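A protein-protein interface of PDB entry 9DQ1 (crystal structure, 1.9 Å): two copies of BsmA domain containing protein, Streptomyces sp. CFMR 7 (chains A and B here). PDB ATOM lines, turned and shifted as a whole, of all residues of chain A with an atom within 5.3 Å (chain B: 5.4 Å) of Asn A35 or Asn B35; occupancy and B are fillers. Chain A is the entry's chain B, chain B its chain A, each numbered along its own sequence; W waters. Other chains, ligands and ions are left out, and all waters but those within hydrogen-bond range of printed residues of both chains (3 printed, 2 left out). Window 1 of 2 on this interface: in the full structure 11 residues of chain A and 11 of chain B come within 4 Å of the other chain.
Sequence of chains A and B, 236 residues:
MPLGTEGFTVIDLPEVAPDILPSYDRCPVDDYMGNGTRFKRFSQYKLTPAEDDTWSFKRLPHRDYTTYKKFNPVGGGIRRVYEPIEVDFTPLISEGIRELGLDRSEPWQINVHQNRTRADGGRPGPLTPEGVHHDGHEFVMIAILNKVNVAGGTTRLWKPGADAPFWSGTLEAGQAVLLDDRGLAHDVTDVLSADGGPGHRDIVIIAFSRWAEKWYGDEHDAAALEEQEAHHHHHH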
ATOM      1  N   ASP A  30       1.536  22.090   0.013  1.00  0.00           N
ATOM      2  CA  ASP A  30       2.544  22.541  -0.938  1.00  0.00           C
ATOM      3  C   ASP A  30       1.920  23.657  -1.773  1.00  0.00           C
ATOM      4  O   ASP A  30       1.009  23.408  -2.574  1.00  0.00           O
ATOM      5  CB  ASP A  30       2.992  21.368  -1.810  1.00  0.00           C
ATOM      6  CG  ASP A  30       4.157  21.711  -2.738  1.00  0.00           C
ATOM      7  OD1 ASP A  30       4.452  22.898  -2.984  1.00  0.00           O
ATOM      8  OD2 ASP A  30       4.793  20.752  -3.229  1.00  0.00           O
ATOM      9  N   ASP A  31       2.390  24.888  -1.571  1.00  0.00           N
ATOM     10  CA  ASP A  31       1.817  26.037  -2.269  1.00  0.00           C
ATOM     11  C   ASP A  31       2.215  26.131  -3.733  1.00  0.00           C
ATOM     12  O   ASP A  31       1.683  26.994  -4.443  1.00  0.00           O
ATOM     13  CB  ASP A  31       2.227  27.328  -1.569  1.00  0.00           C
ATOM     14  CG  ASP A  31       1.601  27.457  -0.203  1.00  0.00           C
ATOM     15  OD1 ASP A  31       0.384  27.215  -0.102  1.00  0.00           O
ATOM     16  OD2 ASP A  31       2.323  27.776   0.759  1.00  0.00           O
ATOM     17  N   TYR A  32       3.132  25.286  -4.206  1.00  0.00           N
ATOM     18  CA  TYR A  32       3.703  25.453  -5.536  1.00  0.00           C
ATOM     19  C   TYR A  32       3.408  24.320  -6.495  1.00  0.00           C
ATOM     20  O   TYR A  32       3.526  24.530  -7.714  1.00  0.00           O
ATOM     21  CB  TYR A  32       5.228  25.604  -5.446  1.00  0.00           C
ATOM     22  CG  TYR A  32       5.657  26.672  -4.461  1.00  0.00           C
ATOM     23  CD1 TYR A  32       5.767  27.998  -4.851  1.00  0.00           C
ATOM     24  CD2 TYR A  32       5.961  26.347  -3.143  1.00  0.00           C
ATOM     25  CE1 TYR A  32       6.168  28.980  -3.952  1.00  0.00           C
ATOM     26  CE2 TYR A  32       6.345  27.325  -2.232  1.00  0.00           C
ATOM     27  CZ  TYR A  32       6.452  28.635  -2.642  1.00  0.00           C
ATOM     28  OH  TYR A  32       6.858  29.611  -1.741  1.00  0.00           O
ATOM     29  N   MET A  33       3.046  23.138  -5.995  1.00  0.00           N
ATOM     30  CA  MET A  33       2.812  21.978  -6.836  1.00  0.00           C
ATOM     31  C   MET A  33       1.610  21.191  -6.355  1.00  0.00           C
ATOM     32  O   MET A  33       1.306  21.157  -5.162  1.00  0.00           O
ATOM     33  CB  MET A  33       3.994  21.030  -6.851  1.00  0.00           C
ATOM     34  CG  MET A  33       4.121  20.371  -8.160  1.00  0.00           C
ATOM     35  SD  MET A  33       5.406  21.323  -8.936  1.00  0.00           S
ATOM     36  CE  MET A  33       6.740  20.645  -7.972  1.00  0.00           C
ATOM     37  N   GLY A  34       0.949  20.527  -7.305  1.00  0.00           N
ATOM     38  CA  GLY A  34      -0.144  19.633  -6.994  1.00  0.00           C
ATOM     39  C   GLY A  34      -1.499  20.286  -6.825  1.00  0.00           C
ATOM     40  O   GLY A  34      -2.481  19.569  -6.586  1.00  0.00           O
ATOM     41  N   ASN A  35      -1.580  21.607  -6.930  1.00  0.00           N
ATOM     42  CA  ASN A  35      -2.852  22.332  -6.919  1.00  0.00           C
ATOM     43  C   ASN A  35      -3.763  21.883  -5.782  1.00  0.00           C
ATOM     44  O   ASN A  35      -4.940  21.537  -5.980  1.00  0.00           O
ATOM     45  CB  ASN A  35      -3.553  22.201  -8.269  1.00  0.00           C
ATOM     46  CG  ASN A  35      -2.887  23.058  -9.324  1.00  0.00           C
ATOM     47  OD1 ASN A  35      -3.094  24.270  -9.358  1.00  0.00           O
ATOM     48  ND2 ASN A  35      -2.064  22.447 -10.160  1.00  0.00           N
ATOM     49  N   GLY A  36      -3.199  21.893  -4.577  1.00  0.00           N
ATOM     50  CA  GLY A  36      -3.934  21.547  -3.384  1.00  0.00           C
ATOM     51  C   GLY A  36      -3.916  20.080  -3.001  1.00  0.00           C
ATOM     52  O   GLY A  36      -4.361  19.753  -1.896  1.00  0.00           O
ATOM     53  N   THR A  37      -3.419  19.186  -3.867  1.00  0.00           N
ATOM     54  CA  THR A  37      -3.391  17.758  -3.554  1.00  0.00           C
ATOM     55  C   THR A  37      -2.129  17.330  -2.814  1.00  0.00           C
ATOM     56  O   THR A  37      -2.062  16.182  -2.367  1.00  0.00           O
ATOM     57  CB  THR A  37      -3.505  16.902  -4.819  1.00  0.00           C
ATOM     58  OG1 THR A  37      -2.328  17.064  -5.620  1.00  0.00           O
ATOM     59  CG2 THR A  37      -4.735  17.287  -5.633  1.00  0.00           C
ATOM     60  N   ARG A 123     -10.974  13.279  -8.340  1.00  0.00           N
ATOM     61  CA  ARG A 123      -9.801  14.148  -8.273  1.00  0.00           C
ATOM     62  C   ARG A 123      -8.551  13.324  -7.980  1.00  0.00           C
ATOM     63  O   ARG A 123      -8.188  13.120  -6.819  1.00  0.00           O
ATOM     64  CB  ARG A 123      -9.976  15.242  -7.224  1.00  0.00           C
ATOM     65  CG  ARG A 123      -8.834  16.300  -7.257  1.00  0.00           C
ATOM     66  CD  ARG A 123      -8.940  17.225  -8.500  1.00  0.00           C
ATOM     67  NE  ARG A 123      -7.758  18.073  -8.664  1.00  0.00           N
ATOM     68  CZ  ARG A 123      -7.504  19.156  -7.943  1.00  0.00           C
ATOM     69  NH1 ARG A 123      -8.376  19.616  -7.057  1.00  0.00           N
ATOM     70  NH2 ARG A 123      -6.342  19.795  -8.110  1.00  0.00           N
ATOM     71  N   ASP B  30      -8.964  29.137  -9.194  1.00  0.00           N
ATOM     72  CA  ASP B  30      -8.932  27.927 -10.013  1.00  0.00           C
ATOM     73  C   ASP B  30      -8.343  26.804  -9.166  1.00  0.00           C
ATOM     74  O   ASP B  30      -7.150  26.822  -8.863  1.00  0.00           O
ATOM     75  CB  ASP B  30      -8.081  28.183 -11.260  1.00  0.00           C
ATOM     76  CG  ASP B  30      -8.193  27.066 -12.321  1.00  0.00           C
ATOM     77  OD1 ASP B  30      -8.506  25.901 -11.986  1.00  0.00           O
ATOM     78  OD2 ASP B  30      -7.952  27.371 -13.509  1.00  0.00           O
ATOM     79  N   ASP B  31      -9.170  25.825  -8.782  1.00  0.00           N
ATOM     80  CA  ASP B  31      -8.699  24.745  -7.916  1.00  0.00           C
ATOM     81  C   ASP B  31      -7.736  23.789  -8.608  1.00  0.00           C
ATOM     82  O   ASP B  31      -7.115  22.958  -7.927  1.00  0.00           O
ATOM     83  CB  ASP B  31      -9.888  23.943  -7.388  1.00  0.00           C
ATOM     84  CG  ASP B  31     -10.680  24.700  -6.342  1.00  0.00           C
ATOM     85  OD1 ASP B  31     -10.060  25.458  -5.570  1.00  0.00           O
ATOM     86  OD2 ASP B  31     -11.919  24.549  -6.295  1.00  0.00           O
ATOM     87  N   TYR B  32      -7.618  23.860  -9.933  1.00  0.00           N
ATOM     88  CA  TYR B  32      -6.955  22.813 -10.700  1.00  0.00           C
ATOM     89  C   TYR B  32      -5.677  23.253 -11.384  1.00  0.00           C
ATOM     90  O   TYR B  32      -4.868  22.392 -11.764  1.00  0.00           O
ATOM     91  CB  TYR B  32      -7.905  22.269 -11.774  1.00  0.00           C
ATOM     92  CG  TYR B  32      -9.238  21.834 -11.217  1.00  0.00           C
ATOM     93  CD1 TYR B  32      -9.420  20.547 -10.727  1.00  0.00           C
ATOM     94  CD2 TYR B  32     -10.315  22.714 -11.172  1.00  0.00           C
ATOM     95  CE1 TYR B  32     -10.654  20.136 -10.217  1.00  0.00           C
ATOM     96  CE2 TYR B  32     -11.546  22.315 -10.653  1.00  0.00           C
ATOM     97  CZ  TYR B  32     -11.709  21.036 -10.178  1.00  0.00           C
ATOM     98  OH  TYR B  32     -12.943  20.663  -9.685  1.00  0.00           O
ATOM     99  N   MET B  33      -5.489  24.552 -11.599  1.00  0.00           N
ATOM    100  CA  MET B  33      -4.329  25.018 -12.345  1.00  0.00           C
ATOM    101  C   MET B  33      -3.809  26.306 -11.745  1.00  0.00           C
ATOM    102  O   MET B  33      -4.571  27.109 -11.198  1.00  0.00           O
ATOM    103  CB  MET B  33      -4.653  25.223 -13.817  1.00  0.00           C
ATOM    104  CG  MET B  33      -4.805  23.896 -14.556  1.00  0.00           C
ATOM    105  SD  MET B  33      -4.934  24.109 -16.314  1.00  0.00           S
ATOM    106  CE  MET B  33      -3.258  24.518 -16.787  1.00  0.00           C
ATOM    107  N   GLY B  34      -2.486  26.482 -11.834  1.00  0.00           N
ATOM    108  CA  GLY B  34      -1.858  27.714 -11.411  1.00  0.00           C
ATOM    109  C   GLY B  34      -1.396  27.744  -9.973  1.00  0.00           C
ATOM    110  O   GLY B  34      -0.812  28.755  -9.553  1.00  0.00           O
ATOM    111  N   ASN B  35      -1.646  26.683  -9.210  1.00  0.00           N
ATOM    112  CA  ASN B  35      -1.229  26.558  -7.815  1.00  0.00           C
ATOM    113  C   ASN B  35      -1.508  27.831  -7.027  1.00  0.00           C
ATOM    114  O   ASN B  35      -0.627  28.432  -6.408  1.00  0.00           O
ATOM    115  CB  ASN B  35       0.234  26.131  -7.722  1.00  0.00           C
ATOM    116  CG  ASN B  35       0.416  24.696  -8.144  1.00  0.00           C
ATOM    117  OD1 ASN B  35       0.170  23.783  -7.356  1.00  0.00           O
ATOM    118  ND2 ASN B  35       0.820  24.483  -9.396  1.00  0.00           N
ATOM    119  N   GLY B  36      -2.777  28.221  -7.046  1.00  0.00           N
ATOM    120  CA  GLY B  36      -3.247  29.364  -6.299  1.00  0.00           C
ATOM    121  C   GLY B  36      -3.031  30.717  -6.955  1.00  0.00           C
ATOM    122  O   GLY B  36      -3.498  31.726  -6.404  1.00  0.00           O
ATOM    123  N   THR B  37      -2.331  30.785  -8.092  1.00  0.00           N
ATOM    124  CA  THR B  37      -2.126  32.061  -8.779  1.00  0.00           C
ATOM    125  C   THR B  37      -3.231  32.396  -9.782  1.00  0.00           C
ATOM    126  O   THR B  37      -3.199  33.489 -10.371  1.00  0.00           O
ATOM    127  CB  THR B  37      -0.792  32.093  -9.544  1.00  0.00           C
ATOM    128  OG1 THR B  37      -0.852  31.191 -10.659  1.00  0.00           O
ATOM    129  CG2 THR B  37       0.432  31.738  -8.639  1.00  0.00           C
ATOM    130  N   ARG B 123       7.111  35.388  -6.951  1.00  0.00           N
ATOM    131  CA  ARG B 123       6.146  34.371  -7.383  1.00  0.00           C
ATOM    132  C   ARG B 123       5.515  34.768  -8.714  1.00  0.00           C
ATOM    133  O   ARG B 123       4.478  35.449  -8.754  1.00  0.00           O
ATOM    134  CB  ARG B 123       5.062  34.154  -6.331  1.00  0.00           C
ATOM    135  CG  ARG B 123       4.096  32.981  -6.671  1.00  0.00           C
ATOM    136  CD  ARG B 123       4.777  31.614  -6.412  1.00  0.00           C
ATOM    137  NE  ARG B 123       3.975  30.511  -6.928  1.00  0.00           N
ATOM    138  CZ  ARG B 123       2.996  29.913  -6.265  1.00  0.00           C
ATOM    139  NH1 ARG B 123       2.675  30.271  -5.032  1.00  0.00           N
ATOM    140  NH2 ARG B 123       2.295  28.954  -6.871  1.00  0.00           N
HETATM  141  O   HOH W   1      -5.278  24.697  -5.729  1.00  0.00           O
HETATM  142  O   HOH W   2      -2.483  21.521 -12.835  1.00  0.00           O
HETATM  143  O   HOH W   3      -0.107  29.695  -3.961  1.00  0.00           O
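The backbone NH (N) of Asn B35 is in hydrogen-bond range of the side-chain amide oxygen (OD1) of Asn A35 (2.8 Å). O of Tyr B32 lies close to ND2 of Asn A35, 3.2 Å away. The backbone carbonyl oxygen (O) of Asp B31 sits close to the backbone carbonyl oxygen (O) of Asn A35 (3.2 Å). The side-chain amide nitrogen (ND2) of Asn B35 sits close to the backbone carbonyl oxygen (O) of Tyr A32 (3.2 Å). OD1 of Asn A35 sits close to N of Met B33 (3.3 Å). OD1 of Asn A35 is in hydrogen-bond range of N of Gly B34 (3.4 Å). The backbone NH (N) of Gly A34 lies within hydrogen-bond range of the side-chain amide oxygen (OD1) of Asn B35. O of Asp B31 lies within hydrogen-bond range of NH2 of Arg A123, 3.3 Å away. The backbone NH (N) of Met A33 lies close to the side-chain amide oxygen (OD1) of Asn B35 (3.2 Å). The backbone carbonyl oxygen (O) of Asp A31 is in hydrogen-bond range of the guanidinium group (NH2) of Arg B123, at 3.2 Å. O of Asn B35 sits close to O of Asp A31, at 3.4 Å.
The side-chain carboxylate (OD1) of Asp B30 lies within hydrogen-bond range of the backbone NH (N) of Tyr B32 (3.0 Å). OG1 of Thr B37 lies within hydrogen-bond range of O of Gly B34, 2.7 Å away. The guanidinium group (NH2) of Arg A123 sits at hydrogen-bond distance from the backbone carbonyl oxygen (O) of Asn A35 (3.1 Å). OG1 of Thr A37 lies within hydrogen-bond range of O of Gly A34, 2.7 Å away. OD1 of Asp B30 lies within hydrogen-bond range of N of Met B33, at 3.3 Å. OD1 of Asp A30 is in hydrogen-bond range of N of Met A33 (3.3 Å).
Among the printed residues, merely in contact across the chains: Arg A123 with Tyr B32 (3.6 Å) and Tyr A32 with Arg B123 (3.7 Å).
Of chain B, only Asp B31 (3.2 Å), Tyr B32 (3.2 Å), Met B33 (3.2 Å), Gly B34 (3.4 Å) and Asn B35 (2.8 Å) come within 4 Å of Asn A35. Printed residues of chain A within 4 Å of Asn B35: Asp A31 (3.4 Å), Tyr A32 (3.1 Å), Met A33 (3.1 Å), Gly A34 (3.3 Å) and Asn A35 (2.8 Å). Printed residues of chain A within 4 Å of Met B33: Asn A35. Printed residues of chain A within 4 Å of Gly B34: Asn A35 (3.4 Å). Of the printed residues of chain A, Asp B31 touches Asn A35 (3.2 Å) and Arg A123 (3.3 Å). Printed residues of chain B within 4 Å of Gly A34: Asn B35. Of the printed residues of chain B, Met A33 touches Asn B35 (3.1 Å).
Of the 9 printed residues of chain A, 6 touch a printed residue of chain B. Printed residues of chain A that touch a printed residue of chain B: Asp A31, Tyr A32, Met A33, Gly A34, Asn A35 and Arg A123. Hydrophobic or aromatic side chains of chain A within 4 Å of the printed part of chain B: Tyr A32. Along chain A the printed residues that touch a printed residue of chain B span positions 31 to 123.
Asp A31 touches Asn B35, and with the chains exchanged Asn A35 touches Asp B31. Tyr A32 touches Asn B35, and with the chains exchanged Asn A35 touches Tyr B32. Met A33 touches Asn B35, and with the chains exchanged Asn A35 touches Met B33. Asn B35 touches its own counterpart, Asn A35. 9 positions are printed for both chains. Of the 13 pairs that touch across the chains among the printed residues, 13 have their exchanged pair printed and touching as well.
Water W2 lies within hydrogen-bond range of O of Tyr B32 and ND2 of Asn A35. Water W3 lies within hydrogen-bond range of the backbone carbonyl oxygen of Asn B35, the guanidinium group of Arg B123 and the backbone carbonyl oxygen of Asp A31. Water W1 lies within hydrogen-bond range of the backbone carbonyl oxygen (O) of Asn A35 (3.2 Å) and the backbone carbonyl oxygen (O) of Asp B31 (3.4 Å).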
